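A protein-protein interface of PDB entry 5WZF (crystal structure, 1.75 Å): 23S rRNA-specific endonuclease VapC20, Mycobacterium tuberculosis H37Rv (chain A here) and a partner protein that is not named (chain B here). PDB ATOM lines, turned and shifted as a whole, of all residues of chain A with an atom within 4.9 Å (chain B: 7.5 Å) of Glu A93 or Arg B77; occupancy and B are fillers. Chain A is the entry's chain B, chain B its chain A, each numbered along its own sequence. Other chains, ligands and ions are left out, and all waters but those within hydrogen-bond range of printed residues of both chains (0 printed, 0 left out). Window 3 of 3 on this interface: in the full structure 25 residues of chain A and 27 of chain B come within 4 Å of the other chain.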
ATOM      1  N   ALA A  89      33.148   2.018 -11.543  1.00  0.00           N
ATOM      2  CA  ALA A  89      32.462   1.105 -12.449  1.00  0.00           C
ATOM      3  C   ALA A  89      32.624  -0.338 -11.987  1.00  0.00           C
ATOM      4  O   ALA A  89      31.674  -1.117 -12.031  1.00  0.00           O
ATOM      5  CB  ALA A  89      32.985   1.267 -13.869  1.00  0.00           C
ATOM      6  N   ASP A  90      33.830  -0.681 -11.543  1.00  0.00           N
ATOM      7  CA  ASP A  90      34.120  -2.019 -11.032  1.00  0.00           C
ATOM      8  C   ASP A  90      33.261  -2.369  -9.826  1.00  0.00           C
ATOM      9  O   ASP A  90      32.723  -3.471  -9.734  1.00  0.00           O
ATOM     10  CB  ASP A  90      35.598  -2.149 -10.651  1.00  0.00           C
ATOM     11  CG  ASP A  90      36.495  -2.357 -11.853  1.00  0.00           C
ATOM     12  OD1 ASP A  90      35.984  -2.790 -12.908  1.00  0.00           O
ATOM     13  OD2 ASP A  90      37.710  -2.094 -11.740  1.00  0.00           O
ATOM     14  N   LEU A  91      33.149  -1.432  -8.891  1.00  0.00           N
ATOM     15  CA  LEU A  91      32.380  -1.668  -7.677  1.00  0.00           C
ATOM     16  C   LEU A  91      30.896  -1.793  -8.006  1.00  0.00           C
ATOM     17  O   LEU A  91      30.200  -2.644  -7.447  1.00  0.00           O
ATOM     18  CB  LEU A  91      32.624  -0.549  -6.661  1.00  0.00           C
ATOM     19  CG  LEU A  91      32.409  -0.893  -5.185  1.00  0.00           C
ATOM     20  CD1 LEU A  91      33.213  -2.123  -4.794  1.00  0.00           C
ATOM     21  CD2 LEU A  91      32.787   0.280  -4.300  1.00  0.00           C
ATOM     22  N   GLU A  92      30.416  -0.962  -8.930  1.00  0.00           N
ATOM     23  CA  GLU A  92      29.031  -1.052  -9.381  1.00  0.00           C
ATOM     24  C   GLU A  92      28.728  -2.416 -10.003  1.00  0.00           C
ATOM     25  O   GLU A  92      27.654  -2.972  -9.791  1.00  0.00           O
ATOM     26  CB  GLU A  92      28.708   0.060 -10.385  1.00  0.00           C
ATOM     27  CG  GLU A  92      28.439   1.402  -9.737  1.00  0.00           C
ATOM     28  CD  GLU A  92      27.760   2.385 -10.674  1.00  0.00           C
ATOM     29  OE1 GLU A  92      27.568   2.049 -11.859  1.00  0.00           O
ATOM     30  OE2 GLU A  92      27.409   3.488 -10.216  1.00  0.00           O
ATOM     31  N   GLU A  93      29.673  -2.956 -10.764  1.00  0.00           N
ATOM     32  CA  GLU A  93      29.454  -4.249 -11.399  1.00  0.00           C
ATOM     33  C   GLU A  93      29.344  -5.345 -10.340  1.00  0.00           C
ATOM     34  O   GLU A  93      28.546  -6.276 -10.477  1.00  0.00           O
ATOM     35  CB  GLU A  93      30.574  -4.566 -12.390  1.00  0.00           C
ATOM     36  CG  GLU A  93      30.441  -5.919 -13.075  1.00  0.00           C
ATOM     37  CD  GLU A  93      29.190  -6.033 -13.931  1.00  0.00           C
ATOM     38  OE1 GLU A  93      28.662  -4.986 -14.366  1.00  0.00           O
ATOM     39  OE2 GLU A  93      28.733  -7.174 -14.161  1.00  0.00           O
ATOM     40  N   GLN A  94      30.133  -5.227  -9.276  1.00  0.00           N
ATOM     41  CA  GLN A  94      30.040  -6.178  -8.174  1.00  0.00           C
ATOM     42  C   GLN A  94      28.688  -6.035  -7.488  1.00  0.00           C
ATOM     43  O   GLN A  94      28.082  -7.025  -7.082  1.00  0.00           O
ATOM     44  CB  GLN A  94      31.168  -5.973  -7.165  1.00  0.00           C
ATOM     45  CG  GLN A  94      31.170  -7.014  -6.054  1.00  0.00           C
ATOM     46  CD  GLN A  94      32.166  -6.703  -4.960  1.00  0.00           C
ATOM     47  OE1 GLN A  94      31.886  -5.913  -4.061  1.00  0.00           O
ATOM     48  NE2 GLN A  94      33.338  -7.325  -5.029  1.00  0.00           N
ATOM     49  N   ALA A  95      28.217  -4.797  -7.370  1.00  0.00           N
ATOM     50  CA  ALA A  95      26.908  -4.529  -6.787  1.00  0.00           C
ATOM     51  C   ALA A  95      25.789  -5.155  -7.615  1.00  0.00           C
ATOM     52  O   ALA A  95      24.830  -5.690  -7.062  1.00  0.00           O
ATOM     53  CB  ALA A  95      26.684  -3.031  -6.649  1.00  0.00           C
ATOM     54  N   TRP A  96      25.909  -5.091  -8.939  1.00  0.00           N
ATOM     55  CA  TRP A  96      24.907  -5.695  -9.814  1.00  0.00           C
ATOM     56  C   TRP A  96      24.882  -7.218  -9.673  1.00  0.00           C
ATOM     57  O   TRP A  96      23.807  -7.824  -9.595  1.00  0.00           O
ATOM     58  CB  TRP A  96      25.158  -5.324 -11.280  1.00  0.00           C
ATOM     59  CG  TRP A  96      24.683  -3.951 -11.682  1.00  0.00           C
ATOM     60  CD1 TRP A  96      25.455  -2.911 -12.113  1.00  0.00           C
ATOM     61  CD2 TRP A  96      23.330  -3.482 -11.706  1.00  0.00           C
ATOM     62  NE1 TRP A  96      24.667  -1.820 -12.398  1.00  0.00           N
ATOM     63  CE2 TRP A  96      23.358  -2.144 -12.155  1.00  0.00           C
ATOM     64  CE3 TRP A  96      22.096  -4.058 -11.379  1.00  0.00           C
ATOM     65  CZ2 TRP A  96      22.203  -1.376 -12.295  1.00  0.00           C
ATOM     66  CZ3 TRP A  96      20.950  -3.294 -11.519  1.00  0.00           C
ATOM     67  CH2 TRP A  96      21.013  -1.967 -11.971  1.00  0.00           C
ATOM     68  N   GLU A  97      26.061  -7.833  -9.659  1.00  0.00           N
ATOM     69  CA  GLU A  97      26.158  -9.282  -9.505  1.00  0.00           C
ATOM     70  C   GLU A  97      25.574  -9.688  -8.160  1.00  0.00           C
ATOM     71  O   GLU A  97      24.893 -10.707  -8.046  1.00  0.00           O
ATOM     72  CB  GLU A  97      27.612  -9.753  -9.623  1.00  0.00           C
ATOM     73  CG  GLU A  97      28.254  -9.451 -10.966  1.00  0.00           C
ATOM     74  CD  GLU A  97      29.725  -9.813 -11.010  1.00  0.00           C
ATOM     75  OE1 GLU A  97      30.257 -10.286  -9.983  1.00  0.00           O
ATOM     76  OE2 GLU A  97      30.352  -9.623 -12.074  1.00  0.00           O
ATOM     77  N   THR B  49      21.732   5.303 -22.058  1.00  0.00           N
ATOM     78  CA  THR B  49      21.165   5.503 -20.730  1.00  0.00           C
ATOM     79  C   THR B  49      22.334   5.668 -19.761  1.00  0.00           C
ATOM     80  O   THR B  49      23.477   5.776 -20.196  1.00  0.00           O
ATOM     81  CB  THR B  49      20.238   4.344 -20.317  1.00  0.00           C
ATOM     82  OG1 THR B  49      19.480   4.726 -19.162  1.00  0.00           O
ATOM     83  CG2 THR B  49      21.041   3.077 -20.024  1.00  0.00           C
ATOM     84  N   ASN B  51      24.218   4.758 -15.648  1.00  0.00           N
ATOM     85  CA  ASN B  51      24.289   3.847 -14.515  1.00  0.00           C
ATOM     86  C   ASN B  51      23.287   4.239 -13.433  1.00  0.00           C
ATOM     87  O   ASN B  51      22.645   3.378 -12.831  1.00  0.00           O
ATOM     88  CB  ASN B  51      25.715   3.796 -13.942  1.00  0.00           C
ATOM     89  CG  ASN B  51      26.234   5.161 -13.504  1.00  0.00           C
ATOM     90  OD1 ASN B  51      25.982   6.181 -14.148  1.00  0.00           O
ATOM     91  ND2 ASN B  51      26.975   5.179 -12.401  1.00  0.00           N
ATOM     92  N   LEU B  54      19.788   3.126 -14.575  1.00  0.00           N
ATOM     93  CA  LEU B  54      19.590   1.683 -14.478  1.00  0.00           C
ATOM     94  C   LEU B  54      19.413   1.273 -13.023  1.00  0.00           C
ATOM     95  O   LEU B  54      18.565   0.443 -12.703  1.00  0.00           O
ATOM     96  CB  LEU B  54      20.754   0.922 -15.114  1.00  0.00           C
ATOM     97  CG  LEU B  54      20.714   0.884 -16.645  1.00  0.00           C
ATOM     98  CD1 LEU B  54      21.774  -0.074 -17.184  1.00  0.00           C
ATOM     99  CD2 LEU B  54      19.321   0.504 -17.134  1.00  0.00           C
ATOM    100  N   VAL B  71      15.826  -8.099 -12.508  1.00  0.00           N
ATOM    101  CA  VAL B  71      16.996  -8.680 -13.164  1.00  0.00           C
ATOM    102  C   VAL B  71      17.017  -8.298 -14.647  1.00  0.00           C
ATOM    103  O   VAL B  71      18.080  -8.073 -15.230  1.00  0.00           O
ATOM    104  CB  VAL B  71      17.027 -10.211 -12.993  1.00  0.00           C
ATOM    105  CG1 VAL B  71      18.065 -10.847 -13.907  1.00  0.00           C
ATOM    106  CG2 VAL B  71      17.315 -10.560 -11.547  1.00  0.00           C
ATOM    107  N   ALA B  72      15.833  -8.193 -15.242  1.00  0.00           N
ATOM    108  CA  ALA B  72      15.713  -7.741 -16.624  1.00  0.00           C
ATOM    109  C   ALA B  72      16.340  -6.362 -16.800  1.00  0.00           C
ATOM    110  O   ALA B  72      17.014  -6.092 -17.794  1.00  0.00           O
ATOM    111  CB  ALA B  72      14.260  -7.720 -17.048  1.00  0.00           C
ATOM    112  N   ALA B  73      16.119  -5.495 -15.818  1.00  0.00           N
ATOM    113  CA  ALA B  73      16.703  -4.163 -15.828  1.00  0.00           C
ATOM    114  C   ALA B  73      18.218  -4.233 -15.659  1.00  0.00           C
ATOM    115  O   ALA B  73      18.958  -3.493 -16.305  1.00  0.00           O
ATOM    116  CB  ALA B  73      16.083  -3.309 -14.736  1.00  0.00           C
ATOM    117  N   ALA B  74      18.672  -5.129 -14.788  1.00  0.00           N
ATOM    118  CA  ALA B  74      20.098  -5.317 -14.560  1.00  0.00           C
ATOM    119  C   ALA B  74      20.807  -5.715 -15.853  1.00  0.00           C
ATOM    120  O   ALA B  74      21.926  -5.280 -16.125  1.00  0.00           O
ATOM    121  CB  ALA B  74      20.327  -6.371 -13.476  1.00  0.00           C
ATOM    122  N   ALA B  75      20.132  -6.527 -16.660  1.00  0.00           N
ATOM    123  CA  ALA B  75      20.732  -7.088 -17.863  1.00  0.00           C
ATOM    124  C   ALA B  75      20.960  -6.046 -18.959  1.00  0.00           C
ATOM    125  O   ALA B  75      21.736  -6.277 -19.887  1.00  0.00           O
ATOM    126  CB  ALA B  75      19.871  -8.204 -18.387  1.00  0.00           C
ATOM    127  N   ILE B  76      20.281  -4.909 -18.858  1.00  0.00           N
ATOM    128  CA  ILE B  76      20.457  -3.830 -19.826  1.00  0.00           C
ATOM    129  C   ILE B  76      21.917  -3.376 -19.856  1.00  0.00           C
ATOM    130  O   ILE B  76      22.453  -3.041 -20.913  1.00  0.00           O
ATOM    131  CB  ILE B  76      19.536  -2.632 -19.506  1.00  0.00           C
ATOM    132  CG1 ILE B  76      18.072  -3.054 -19.617  1.00  0.00           C
ATOM    133  CG2 ILE B  76      19.813  -1.468 -20.450  1.00  0.00           C
ATOM    134  CD1 ILE B  76      17.083  -1.992 -19.176  1.00  0.00           C
ATOM    135  N   ARG B  77      22.572  -3.409 -18.699  1.00  0.00           N
ATOM    136  CA  ARG B  77      23.973  -3.006 -18.606  1.00  0.00           C
ATOM    137  C   ARG B  77      24.872  -3.897 -19.457  1.00  0.00           C
ATOM    138  O   ARG B  77      25.994  -3.516 -19.791  1.00  0.00           O
ATOM    139  CB  ARG B  77      24.448  -3.031 -17.152  1.00  0.00           C
ATOM    140  CG  ARG B  77      24.975  -4.383 -16.687  1.00  0.00           C
ATOM    141  CD  ARG B  77      25.190  -4.402 -15.178  1.00  0.00           C
ATOM    142  NE  ARG B  77      25.861  -5.616 -14.726  1.00  0.00           N
ATOM    143  CZ  ARG B  77      25.254  -6.786 -14.556  1.00  0.00           C
ATOM    144  NH1 ARG B  77      23.957  -6.906 -14.806  1.00  0.00           N
ATOM    145  NH2 ARG B  77      25.943  -7.840 -14.141  1.00  0.00           N
ATOM    146  N   LEU B  78      24.371  -5.082 -19.806  1.00  0.00           N
ATOM    147  CA  LEU B  78      25.122  -6.047 -20.601  1.00  0.00           C
ATOM    148  C   LEU B  78      24.859  -5.887 -22.096  1.00  0.00           C
ATOM    149  O   LEU B  78      25.484  -6.556 -22.919  1.00  0.00           O
ATOM    150  CB  LEU B  78      24.769  -7.478 -20.184  1.00  0.00           C
ATOM    151  CG  LEU B  78      24.771  -7.839 -18.696  1.00  0.00           C
ATOM    152  CD1 LEU B  78      24.322  -9.276 -18.517  1.00  0.00           C
ATOM    153  CD2 LEU B  78      26.145  -7.641 -18.093  1.00  0.00           C
ATOM    154  N   SER B  79      23.929  -5.004 -22.441  1.00  0.00           N
ATOM    155  CA  SER B  79      23.484  -4.869 -23.827  1.00  0.00           C
ATOM    156  C   SER B  79      24.588  -4.367 -24.746  1.00  0.00           C
ATOM    157  O   SER B  79      25.400  -3.526 -24.364  1.00  0.00           O
ATOM    158  CB  SER B  79      22.284  -3.929 -23.915  1.00  0.00           C
ATOM    159  OG  SER B  79      21.873  -3.771 -25.261  1.00  0.00           O
ATOM    160  N   THR B  80      24.607  -4.897 -25.962  1.00  0.00           N
ATOM    161  CA  THR B  80      25.546  -4.447 -26.978  1.00  0.00           C
ATOM    162  C   THR B  80      24.949  -3.308 -27.799  1.00  0.00           C
ATOM    163  O   THR B  80      25.643  -2.680 -28.599  1.00  0.00           O
ATOM    164  CB  THR B  80      25.937  -5.592 -27.923  1.00  0.00           C
ATOM    165  OG1 THR B  80      24.746  -6.188 -28.453  1.00  0.00           O
ATOM    166  CG2 THR B  80      26.753  -6.656 -27.186  1.00  0.00           C
ATOM    167  N   VAL B  82      22.527  -0.986 -26.291  1.00  0.00           N
ATOM    168  CA  VAL B  82      22.257   0.154 -25.425  1.00  0.00           C
ATOM    169  C   VAL B  82      23.573   0.621 -24.824  1.00  0.00           C
ATOM    170  O   VAL B  82      24.292  -0.165 -24.209  1.00  0.00           O
ATOM    171  CB  VAL B  82      21.261  -0.187 -24.294  1.00  0.00           C
ATOM    172  CG1 VAL B  82      21.011   1.043 -23.406  1.00  0.00           C
ATOM    173  CG2 VAL B  82      19.957  -0.716 -24.874  1.00  0.00           C
ATOM    174  N   ARG B  83      23.901   1.892 -25.015  1.00  0.00           N
ATOM    175  CA  ARG B  83      25.127   2.435 -24.440  1.00  0.00           C
ATOM    176  C   ARG B  83      24.858   2.941 -23.030  1.00  0.00           C
ATOM    177  O   ARG B  83      24.084   3.875 -22.834  1.00  0.00           O
ATOM    178  CB  ARG B  83      25.694   3.559 -25.309  1.00  0.00           C
ATOM    179  CG  ARG B  83      27.135   3.920 -24.972  1.00  0.00           C
ATOM    180  CD  ARG B  83      27.605   5.131 -25.761  1.00  0.00           C
ATOM    181  NE  ARG B  83      29.062   5.243 -25.793  1.00  0.00           N
ATOM    182  CZ  ARG B  83      29.800   5.077 -26.887  1.00  0.00           C
ATOM    183  NH1 ARG B  83      29.218   4.786 -28.044  1.00  0.00           N
ATOM    184  NH2 ARG B  83      31.119   5.198 -26.825  1.00  0.00           N
ATOM    185  N   VAL B  84      25.496   2.318 -22.049  1.00  0.00           N
ATOM    186  CA  VAL B  84      25.301   2.704 -20.659  1.00  0.00           C
ATOM    187  C   VAL B  84      26.457   3.577 -20.194  1.00  0.00           C
ATOM    188  O   VAL B  84      27.578   3.101 -20.029  1.00  0.00           O
ATOM    189  CB  VAL B  84      25.182   1.479 -19.736  1.00  0.00           C
ATOM    190  CG1 VAL B  84      24.776   1.907 -18.330  1.00  0.00           C
ATOM    191  CG2 VAL B  84      24.179   0.484 -20.308  1.00  0.00           C
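The guanidinium group (NH2) of Arg B77 lies within salt-bridge range of the side-chain carboxylate (OE2) of Glu A93 (2.9 Å).
The side-chain amide nitrogen of Asn B51 is in hydrogen-bond range of the side-chain carboxylate of Glu A92, at 2.8 Å.
O of Ala B74 sits at hydrogen-bond distance from NH1 of Arg B77, 2.9 Å away.
CH2 of Trp A96 touches O of Leu B54, at 3.5 Å.
CE3 of Trp A96 touches CB of Ala B74 (3.6 Å).
Arg B77 touches Trp A96 (CD to CD1, 3.4 Å).
Glu A93 touches just one residue of chain B: Arg B77 (2.9 Å).
Arg B77 touches just these residues of chain A: Glu A93 (2.9 Å) and Trp A96 (3.4 Å).
Of the printed residues of chain A, Leu B54 touches Trp A96 (3.5 Å).
Of the printed residues of chain B, Trp A96 touches Leu B54, Ala B74 and Arg B77.
Of the printed residues of chain B, Glu A92 touches Asn B51 (2.8 Å).
Of the printed residues of chain A, Ala B74 touches Trp A96.
Arg B83 touches none of the printed residues of chain A.
Val B84 touches none of the printed residues of chain A.
Hydrophobic or aromatic side chains of chain B that line the printed part of chain A: Leu B54 and Ala B74.
Of the 9 printed residues of chain A, 3 touch a printed residue of chain B.
Hydrophobic or aromatic side chains of chain A within 4 Å of the printed part of chain B: Trp A96.
Among the printed residues, 5 pairs touch across the chains.
Among the printed residues, Asp or Glu carboxylates within 4 Å of a Lys or Arg side-chain nitrogen of the other chain: Glu A93 with Arg B77 (2.9 Å).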
